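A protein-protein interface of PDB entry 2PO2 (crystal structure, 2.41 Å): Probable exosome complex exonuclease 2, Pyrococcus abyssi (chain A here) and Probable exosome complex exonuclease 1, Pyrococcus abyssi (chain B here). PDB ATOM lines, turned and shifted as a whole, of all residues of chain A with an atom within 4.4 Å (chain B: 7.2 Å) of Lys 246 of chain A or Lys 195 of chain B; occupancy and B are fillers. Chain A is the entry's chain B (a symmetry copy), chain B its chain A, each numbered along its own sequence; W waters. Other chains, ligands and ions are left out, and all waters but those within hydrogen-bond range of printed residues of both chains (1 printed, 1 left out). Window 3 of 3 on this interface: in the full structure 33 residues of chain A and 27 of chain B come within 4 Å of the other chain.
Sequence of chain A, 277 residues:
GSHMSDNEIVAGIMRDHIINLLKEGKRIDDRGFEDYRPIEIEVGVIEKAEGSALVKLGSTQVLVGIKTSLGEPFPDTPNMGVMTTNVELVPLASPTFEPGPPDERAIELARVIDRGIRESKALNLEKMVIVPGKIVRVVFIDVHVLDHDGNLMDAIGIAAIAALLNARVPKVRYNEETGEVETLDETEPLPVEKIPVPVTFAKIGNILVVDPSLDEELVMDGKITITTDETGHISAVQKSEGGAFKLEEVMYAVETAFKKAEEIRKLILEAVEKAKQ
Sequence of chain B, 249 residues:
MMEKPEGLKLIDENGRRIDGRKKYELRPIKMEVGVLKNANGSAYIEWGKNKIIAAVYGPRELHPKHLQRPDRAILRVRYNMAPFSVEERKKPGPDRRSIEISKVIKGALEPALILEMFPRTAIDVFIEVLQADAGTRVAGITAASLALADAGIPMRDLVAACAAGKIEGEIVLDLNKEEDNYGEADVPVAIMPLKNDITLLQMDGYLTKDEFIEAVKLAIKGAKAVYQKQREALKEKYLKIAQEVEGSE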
ATOM      1  N   LYS A 203     -23.763 -11.219  -9.502  1.00  0.00           N
ATOM      2  CA  LYS A 203     -22.885 -12.107  -8.809  1.00  0.00           C
ATOM      3  C   LYS A 203     -22.615 -11.557  -7.418  1.00  0.00           C
ATOM      4  O   LYS A 203     -22.165 -10.411  -7.243  1.00  0.00           O
ATOM      5  CB  LYS A 203     -21.576 -12.263  -9.560  1.00  0.00           C
ATOM      6  CG  LYS A 203     -20.675 -13.308  -8.969  1.00  0.00           C
ATOM      7  CD  LYS A 203     -19.626 -13.635  -9.963  1.00  0.00           C
ATOM      8  CE  LYS A 203     -18.485 -14.287  -9.318  1.00  0.00           C
ATOM      9  NZ  LYS A 203     -17.612 -14.868 -10.391  1.00  0.00           N
ATOM     10  N   PHE A 245     -16.522 -12.742 -13.794  1.00  0.00           N
ATOM     11  CA  PHE A 245     -17.276 -13.985 -13.976  1.00  0.00           C
ATOM     12  C   PHE A 245     -16.367 -15.037 -14.541  1.00  0.00           C
ATOM     13  O   PHE A 245     -15.460 -14.732 -15.304  1.00  0.00           O
ATOM     14  CB  PHE A 245     -18.457 -13.775 -14.919  1.00  0.00           C
ATOM     15  CG  PHE A 245     -19.541 -12.955 -14.336  1.00  0.00           C
ATOM     16  CD1 PHE A 245     -20.660 -13.549 -13.822  1.00  0.00           C
ATOM     17  CD2 PHE A 245     -19.413 -11.591 -14.241  1.00  0.00           C
ATOM     18  CE1 PHE A 245     -21.649 -12.781 -13.235  1.00  0.00           C
ATOM     19  CE2 PHE A 245     -20.408 -10.832 -13.688  1.00  0.00           C
ATOM     20  CZ  PHE A 245     -21.543 -11.441 -13.201  1.00  0.00           C
ATOM     21  N   LYS A 246     -16.634 -16.282 -14.172  1.00  0.00           N
ATOM     22  CA  LYS A 246     -15.973 -17.407 -14.781  1.00  0.00           C
ATOM     23  C   LYS A 246     -16.714 -17.696 -16.069  1.00  0.00           C
ATOM     24  O   LYS A 246     -17.901 -17.376 -16.195  1.00  0.00           O
ATOM     25  CB  LYS A 246     -15.989 -18.601 -13.843  1.00  0.00           C
ATOM     26  CG  LYS A 246     -15.335 -18.350 -12.504  1.00  0.00           C
ATOM     27  CD  LYS A 246     -13.839 -18.323 -12.626  1.00  0.00           C
ATOM     28  CE  LYS A 246     -13.207 -17.821 -11.328  1.00  0.00           C
ATOM     29  NZ  LYS A 246     -11.769 -18.058 -11.443  1.00  0.00           N
ATOM     30  N   LEU A 247     -16.005 -18.238 -17.050  1.00  0.00           N
ATOM     31  CA  LEU A 247     -16.607 -18.536 -18.344  1.00  0.00           C
ATOM     32  C   LEU A 247     -17.941 -19.282 -18.142  1.00  0.00           C
ATOM     33  O   LEU A 247     -18.912 -19.035 -18.865  1.00  0.00           O
ATOM     34  CB  LEU A 247     -15.642 -19.370 -19.189  1.00  0.00           C
ATOM     35  CG  LEU A 247     -15.771 -19.647 -20.703  1.00  0.00           C
ATOM     36  CD1 LEU A 247     -15.761 -21.102 -21.041  1.00  0.00           C
ATOM     37  CD2 LEU A 247     -16.885 -18.931 -21.382  1.00  0.00           C
ATOM     38  N   GLU A 248     -17.967 -20.184 -17.152  1.00  0.00           N
ATOM     39  CA  GLU A 248     -19.045 -21.138 -16.986  1.00  0.00           C
ATOM     40  C   GLU A 248     -20.128 -20.531 -16.177  1.00  0.00           C
ATOM     41  O   GLU A 248     -21.125 -21.175 -15.918  1.00  0.00           O
ATOM     42  CB  GLU A 248     -18.588 -22.462 -16.362  1.00  0.00           C
ATOM     43  CG  GLU A 248     -17.548 -22.368 -15.284  1.00  0.00           C
ATOM     44  CD  GLU A 248     -16.114 -22.338 -15.833  1.00  0.00           C
ATOM     45  OE1 GLU A 248     -15.708 -23.272 -16.625  1.00  0.00           O
ATOM     46  OE2 GLU A 248     -15.386 -21.385 -15.431  1.00  0.00           O
ATOM     47  N   GLU A 249     -19.934 -19.283 -15.766  1.00  0.00           N
ATOM     48  CA  GLU A 249     -20.976 -18.537 -15.069  1.00  0.00           C
ATOM     49  C   GLU A 249     -21.758 -17.792 -16.121  1.00  0.00           C
ATOM     50  O   GLU A 249     -22.983 -17.675 -16.077  1.00  0.00           O
ATOM     51  CB  GLU A 249     -20.354 -17.603 -14.050  1.00  0.00           C
ATOM     52  CG  GLU A 249     -20.209 -18.243 -12.669  1.00  0.00           C
ATOM     53  CD  GLU A 249     -19.343 -17.429 -11.719  1.00  0.00           C
ATOM     54  OE1 GLU A 249     -18.794 -16.384 -12.115  1.00  0.00           O
ATOM     55  OE2 GLU A 249     -19.200 -17.841 -10.559  1.00  0.00           O
ATOM     56  N   VAL A 250     -21.009 -17.309 -17.092  1.00  0.00           N
ATOM     57  CA  VAL A 250     -21.544 -16.787 -18.335  1.00  0.00           C
ATOM     58  C   VAL A 250     -22.431 -17.834 -19.041  1.00  0.00           C
ATOM     59  O   VAL A 250     -23.599 -17.600 -19.292  1.00  0.00           O
ATOM     60  CB  VAL A 250     -20.380 -16.260 -19.233  1.00  0.00           C
ATOM     61  CG1 VAL A 250     -20.909 -15.779 -20.592  1.00  0.00           C
ATOM     62  CG2 VAL A 250     -19.678 -15.165 -18.492  1.00  0.00           C
ATOM     63  N   ARG B 156      -3.902  -7.735  -8.494  1.00  0.00           N
ATOM     64  CA  ARG B 156      -4.038  -9.172  -8.312  1.00  0.00           C
ATOM     65  C   ARG B 156      -3.579  -9.891  -9.567  1.00  0.00           C
ATOM     66  O   ARG B 156      -3.295 -11.088  -9.569  1.00  0.00           O
ATOM     67  CB  ARG B 156      -5.499  -9.518  -8.091  1.00  0.00           C
ATOM     68  CG  ARG B 156      -6.234  -8.530  -7.296  1.00  0.00           C
ATOM     69  CD  ARG B 156      -7.508  -9.147  -6.812  1.00  0.00           C
ATOM     70  NE  ARG B 156      -7.855  -8.695  -5.464  1.00  0.00           N
ATOM     71  CZ  ARG B 156      -8.517  -7.572  -5.200  1.00  0.00           C
ATOM     72  NH1 ARG B 156      -8.788  -7.264  -3.959  1.00  0.00           N
ATOM     73  NH2 ARG B 156      -8.887  -6.750  -6.168  1.00  0.00           N
ATOM     74  N   ASP B 157      -3.572  -9.138 -10.654  1.00  0.00           N
ATOM     75  CA  ASP B 157      -3.334  -9.680 -11.961  1.00  0.00           C
ATOM     76  C   ASP B 157      -3.416  -8.481 -12.866  1.00  0.00           C
ATOM     77  O   ASP B 157      -4.096  -7.497 -12.553  1.00  0.00           O
ATOM     78  CB  ASP B 157      -4.439 -10.655 -12.342  1.00  0.00           C
ATOM     79  CG  ASP B 157      -3.975 -11.733 -13.320  1.00  0.00           C
ATOM     80  OD1 ASP B 157      -2.879 -11.620 -13.916  1.00  0.00           O
ATOM     81  OD2 ASP B 157      -4.705 -12.735 -13.466  1.00  0.00           O
ATOM     82  N   ILE B 191     -10.152 -10.293 -19.253  1.00  0.00           N
ATOM     83  CA  ILE B 191      -9.984 -11.271 -18.225  1.00  0.00           C
ATOM     84  C   ILE B 191      -8.747 -10.908 -17.471  1.00  0.00           C
ATOM     85  O   ILE B 191      -7.858 -10.279 -18.025  1.00  0.00           O
ATOM     86  CB  ILE B 191      -9.700 -12.683 -18.794  1.00  0.00           C
ATOM     87  CG1 ILE B 191      -9.029 -12.601 -20.163  1.00  0.00           C
ATOM     88  CG2 ILE B 191     -10.954 -13.516 -18.844  1.00  0.00           C
ATOM     89  CD1 ILE B 191      -7.552 -12.904 -20.083  1.00  0.00           C
ATOM     90  N   MET B 192      -8.690 -11.316 -16.213  1.00  0.00           N
ATOM     91  CA  MET B 192      -7.459 -11.433 -15.486  1.00  0.00           C
ATOM     92  C   MET B 192      -7.111 -12.907 -15.653  1.00  0.00           C
ATOM     93  O   MET B 192      -7.798 -13.744 -15.085  1.00  0.00           O
ATOM     94  CB  MET B 192      -7.682 -11.114 -14.024  1.00  0.00           C
ATOM     95  CG  MET B 192      -8.213  -9.749 -13.772  1.00  0.00           C
ATOM     96  SD  MET B 192      -8.562  -9.471 -12.023  1.00  0.00           S
ATOM     97  CE  MET B 192     -10.219 -10.135 -11.921  1.00  0.00           C
ATOM     98  N   PRO B 193      -6.055 -13.222 -16.437  1.00  0.00           N
ATOM     99  CA  PRO B 193      -5.745 -14.551 -16.969  1.00  0.00           C
ATOM    100  C   PRO B 193      -5.420 -15.584 -15.916  1.00  0.00           C
ATOM    101  O   PRO B 193      -5.846 -16.731 -16.041  1.00  0.00           O
ATOM    102  CB  PRO B 193      -4.487 -14.318 -17.819  1.00  0.00           C
ATOM    103  CG  PRO B 193      -4.441 -12.900 -18.055  1.00  0.00           C
ATOM    104  CD  PRO B 193      -5.054 -12.239 -16.867  1.00  0.00           C
ATOM    105  N   LEU B 194      -4.658 -15.199 -14.889  1.00  0.00           N
ATOM    106  CA  LEU B 194      -4.150 -16.141 -13.901  1.00  0.00           C
ATOM    107  C   LEU B 194      -5.263 -16.958 -13.254  1.00  0.00           C
ATOM    108  O   LEU B 194      -5.148 -18.201 -13.100  1.00  0.00           O
ATOM    109  CB  LEU B 194      -3.290 -15.418 -12.867  1.00  0.00           C
ATOM    110  CG  LEU B 194      -1.851 -15.129 -13.311  1.00  0.00           C
ATOM    111  CD1 LEU B 194      -1.080 -14.366 -12.222  1.00  0.00           C
ATOM    112  CD2 LEU B 194      -1.119 -16.430 -13.669  1.00  0.00           C
ATOM    113  N   LYS B 195      -6.356 -16.283 -12.922  1.00  0.00           N
ATOM    114  CA  LYS B 195      -7.477 -16.942 -12.287  1.00  0.00           C
ATOM    115  C   LYS B 195      -8.640 -17.114 -13.248  1.00  0.00           C
ATOM    116  O   LYS B 195      -9.672 -17.628 -12.862  1.00  0.00           O
ATOM    117  CB  LYS B 195      -7.903 -16.191 -11.019  1.00  0.00           C
ATOM    118  CG  LYS B 195      -7.706 -16.935  -9.712  1.00  0.00           C
ATOM    119  CD  LYS B 195      -6.552 -16.401  -8.894  1.00  0.00           C
ATOM    120  CE  LYS B 195      -6.759 -16.612  -7.385  1.00  0.00           C
ATOM    121  NZ  LYS B 195      -7.775 -15.622  -6.872  1.00  0.00           N
ATOM    122  N   ASN B 196      -8.468 -16.704 -14.499  1.00  0.00           N
ATOM    123  CA  ASN B 196      -9.508 -16.855 -15.520  1.00  0.00           C
ATOM    124  C   ASN B 196     -10.796 -16.126 -15.232  1.00  0.00           C
ATOM    125  O   ASN B 196     -11.879 -16.688 -15.472  1.00  0.00           O
ATOM    126  CB  ASN B 196      -9.895 -18.316 -15.717  1.00  0.00           C
ATOM    127  CG  ASN B 196      -8.938 -19.055 -16.590  1.00  0.00           C
ATOM    128  OD1 ASN B 196      -8.306 -20.021 -16.138  1.00  0.00           O
ATOM    129  ND2 ASN B 196      -8.813 -18.620 -17.851  1.00  0.00           N
ATOM    130  N   ASP B 197     -10.674 -14.882 -14.769  1.00  0.00           N
ATOM    131  CA  ASP B 197     -11.780 -14.120 -14.249  1.00  0.00           C
ATOM    132  C   ASP B 197     -12.113 -13.102 -15.293  1.00  0.00           C
ATOM    133  O   ASP B 197     -11.281 -12.252 -15.592  1.00  0.00           O
ATOM    134  CB  ASP B 197     -11.334 -13.399 -12.966  1.00  0.00           C
ATOM    135  CG  ASP B 197     -11.451 -14.276 -11.734  1.00  0.00           C
ATOM    136  OD1 ASP B 197     -12.439 -15.041 -11.692  1.00  0.00           O
ATOM    137  OD2 ASP B 197     -10.578 -14.214 -10.819  1.00  0.00           O
ATOM    138  N   ILE B 198     -13.319 -13.163 -15.851  1.00  0.00           N
ATOM    139  CA  ILE B 198     -13.699 -12.277 -16.912  1.00  0.00           C
ATOM    140  C   ILE B 198     -14.218 -10.990 -16.275  1.00  0.00           C
ATOM    141  O   ILE B 198     -15.216 -11.011 -15.545  1.00  0.00           O
ATOM    142  CB  ILE B 198     -14.798 -12.892 -17.789  1.00  0.00           C
ATOM    143  CG1 ILE B 198     -14.341 -14.218 -18.412  1.00  0.00           C
ATOM    144  CG2 ILE B 198     -15.333 -11.862 -18.799  1.00  0.00           C
ATOM    145  CD1 ILE B 198     -15.470 -15.156 -18.654  1.00  0.00           C
ATOM    146  N   LEU B 201     -17.142  -8.261 -20.434  1.00  0.00           N
ATOM    147  CA  LEU B 201     -17.741  -9.145 -21.413  1.00  0.00           C
ATOM    148  C   LEU B 201     -18.866  -8.400 -22.086  1.00  0.00           C
ATOM    149  O   LEU B 201     -19.847  -8.077 -21.452  1.00  0.00           O
ATOM    150  CB  LEU B 201     -18.233 -10.464 -20.775  1.00  0.00           C
ATOM    151  CG  LEU B 201     -18.111 -11.702 -21.656  1.00  0.00           C
ATOM    152  CD1 LEU B 201     -18.904 -12.913 -21.154  1.00  0.00           C
ATOM    153  CD2 LEU B 201     -18.512 -11.398 -23.049  1.00  0.00           C
ATOM    154  N   ILE B 220     -10.828 -14.971 -25.228  1.00  0.00           N
ATOM    155  CA  ILE B 220     -10.000 -15.255 -24.077  1.00  0.00           C
ATOM    156  C   ILE B 220      -8.681 -15.899 -24.551  1.00  0.00           C
ATOM    157  O   ILE B 220      -7.634 -15.551 -24.041  1.00  0.00           O
ATOM    158  CB  ILE B 220     -10.711 -16.121 -22.970  1.00  0.00           C
ATOM    159  CG1 ILE B 220     -11.997 -15.457 -22.439  1.00  0.00           C
ATOM    160  CG2 ILE B 220      -9.774 -16.417 -21.839  1.00  0.00           C
ATOM    161  CD1 ILE B 220     -12.940 -16.469 -21.753  1.00  0.00           C
ATOM    162  N   TYR B 227      -1.701 -10.977 -22.926  1.00  0.00           N
ATOM    163  CA  TYR B 227      -1.194 -10.986 -21.593  1.00  0.00           C
ATOM    164  C   TYR B 227       0.311 -11.282 -21.567  1.00  0.00           C
ATOM    165  O   TYR B 227       1.078 -10.666 -20.821  1.00  0.00           O
ATOM    166  CB  TYR B 227      -2.020 -11.965 -20.809  1.00  0.00           C
ATOM    167  CG  TYR B 227      -1.612 -12.181 -19.388  1.00  0.00           C
ATOM    168  CD1 TYR B 227      -1.882 -11.207 -18.408  1.00  0.00           C
ATOM    169  CD2 TYR B 227      -1.015 -13.414 -18.994  1.00  0.00           C
ATOM    170  CE1 TYR B 227      -1.528 -11.437 -17.069  1.00  0.00           C
ATOM    171  CE2 TYR B 227      -0.673 -13.645 -17.680  1.00  0.00           C
ATOM    172  CZ  TYR B 227      -0.920 -12.657 -16.715  1.00  0.00           C
ATOM    173  OH  TYR B 227      -0.571 -12.881 -15.396  1.00  0.00           O
HETATM  174  O   HOH W   1     -13.218 -18.558 -16.864  1.00  0.00           O
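Lys 246 of chain A touches just these residues of chain B: Lys 195, Asn 196, Asp 197 and Ile 198.
Of chain A, only Lys 246 comes within 4 Å of Lys 195 of chain B.
Of the printed residues of chain A, Ile 198 of chain B touches Phe 245, Lys 246 and Leu 247.
Of the printed residues of chain B, Leu 247 of chain A touches Ile 198 (3.5 Å).
Of the printed residues of chain B, Phe 245 of chain A touches Asp 197 (3.7 Å) and Ile 198 (2.7 Å).
Of the printed residues of chain A, Asn 196 of chain B touches Lys 246.
Printed residues of chain A within 4 Å of Leu 201 of chain B: Val 250.
Glu 249 of chain A touches none of the printed residues of chain B.
The nearest residue of chain B that does not touch Lys 246 of chain A is Leu 201 of chain B (6.7 Å).
The nearest printed residue of chain A that does not touch Asn 196 of chain B is Phe 245 of chain A (4.1 Å).
Of the 7 printed residues of chain A, 4 touch a printed residue of chain B.
Of the 13 printed residues of chain B, 5 touch a printed residue of chain A.
Among the printed residues, 8 pairs touch across the chains.
Among the printed residues, Asp or Glu carboxylates within 4 Å of a Lys or Arg side-chain nitrogen of the other chain: Lys 246 of chain A with Asp 197 of chain B (3.1 Å).
Phe 245 of chain A touches Asp 197 of chain B (O to C, 3.7 Å).
Asn 196 of chain B touches Lys 246 of chain A.
Ile 198 of chain B touches Lys 246 of chain A (CD1 to C, 3.8 Å).
Leu 247 of chain A touches Ile 198 of chain B (N to CD1, 3.5 Å).
CG1 of Val 250 of chain A touches CD1 of Leu 201 of chain B, at 3.5 Å.
The backbone carbonyl oxygen of Lys 195 of chain B is in hydrogen-bond range of the side-chain amino group of Lys 246 of chain A, at 2.6 Å.
The backbone NH of Ile 198 of chain B sits at hydrogen-bond distance from the backbone carbonyl oxygen of Phe 245 of chain A (2.7 Å).
OD1 of Asp 197 of chain B lies within salt-bridge range of NZ of Lys 246 of chain A (3.1 Å).
The backbone NH (N) of Met 192 of chain B is in hydrogen-bond range of the backbone carbonyl oxygen (O) of Asp 197 of chain B (2.8 Å).
The side-chain carboxylate of Glu 249 of chain A sits at hydrogen-bond distance from the backbone NH of Lys 246 of chain A.
Water W1 bridges O of Asn 196 of chain B (2.7 Å) and N of Leu 247 of chain A (2.8 Å).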
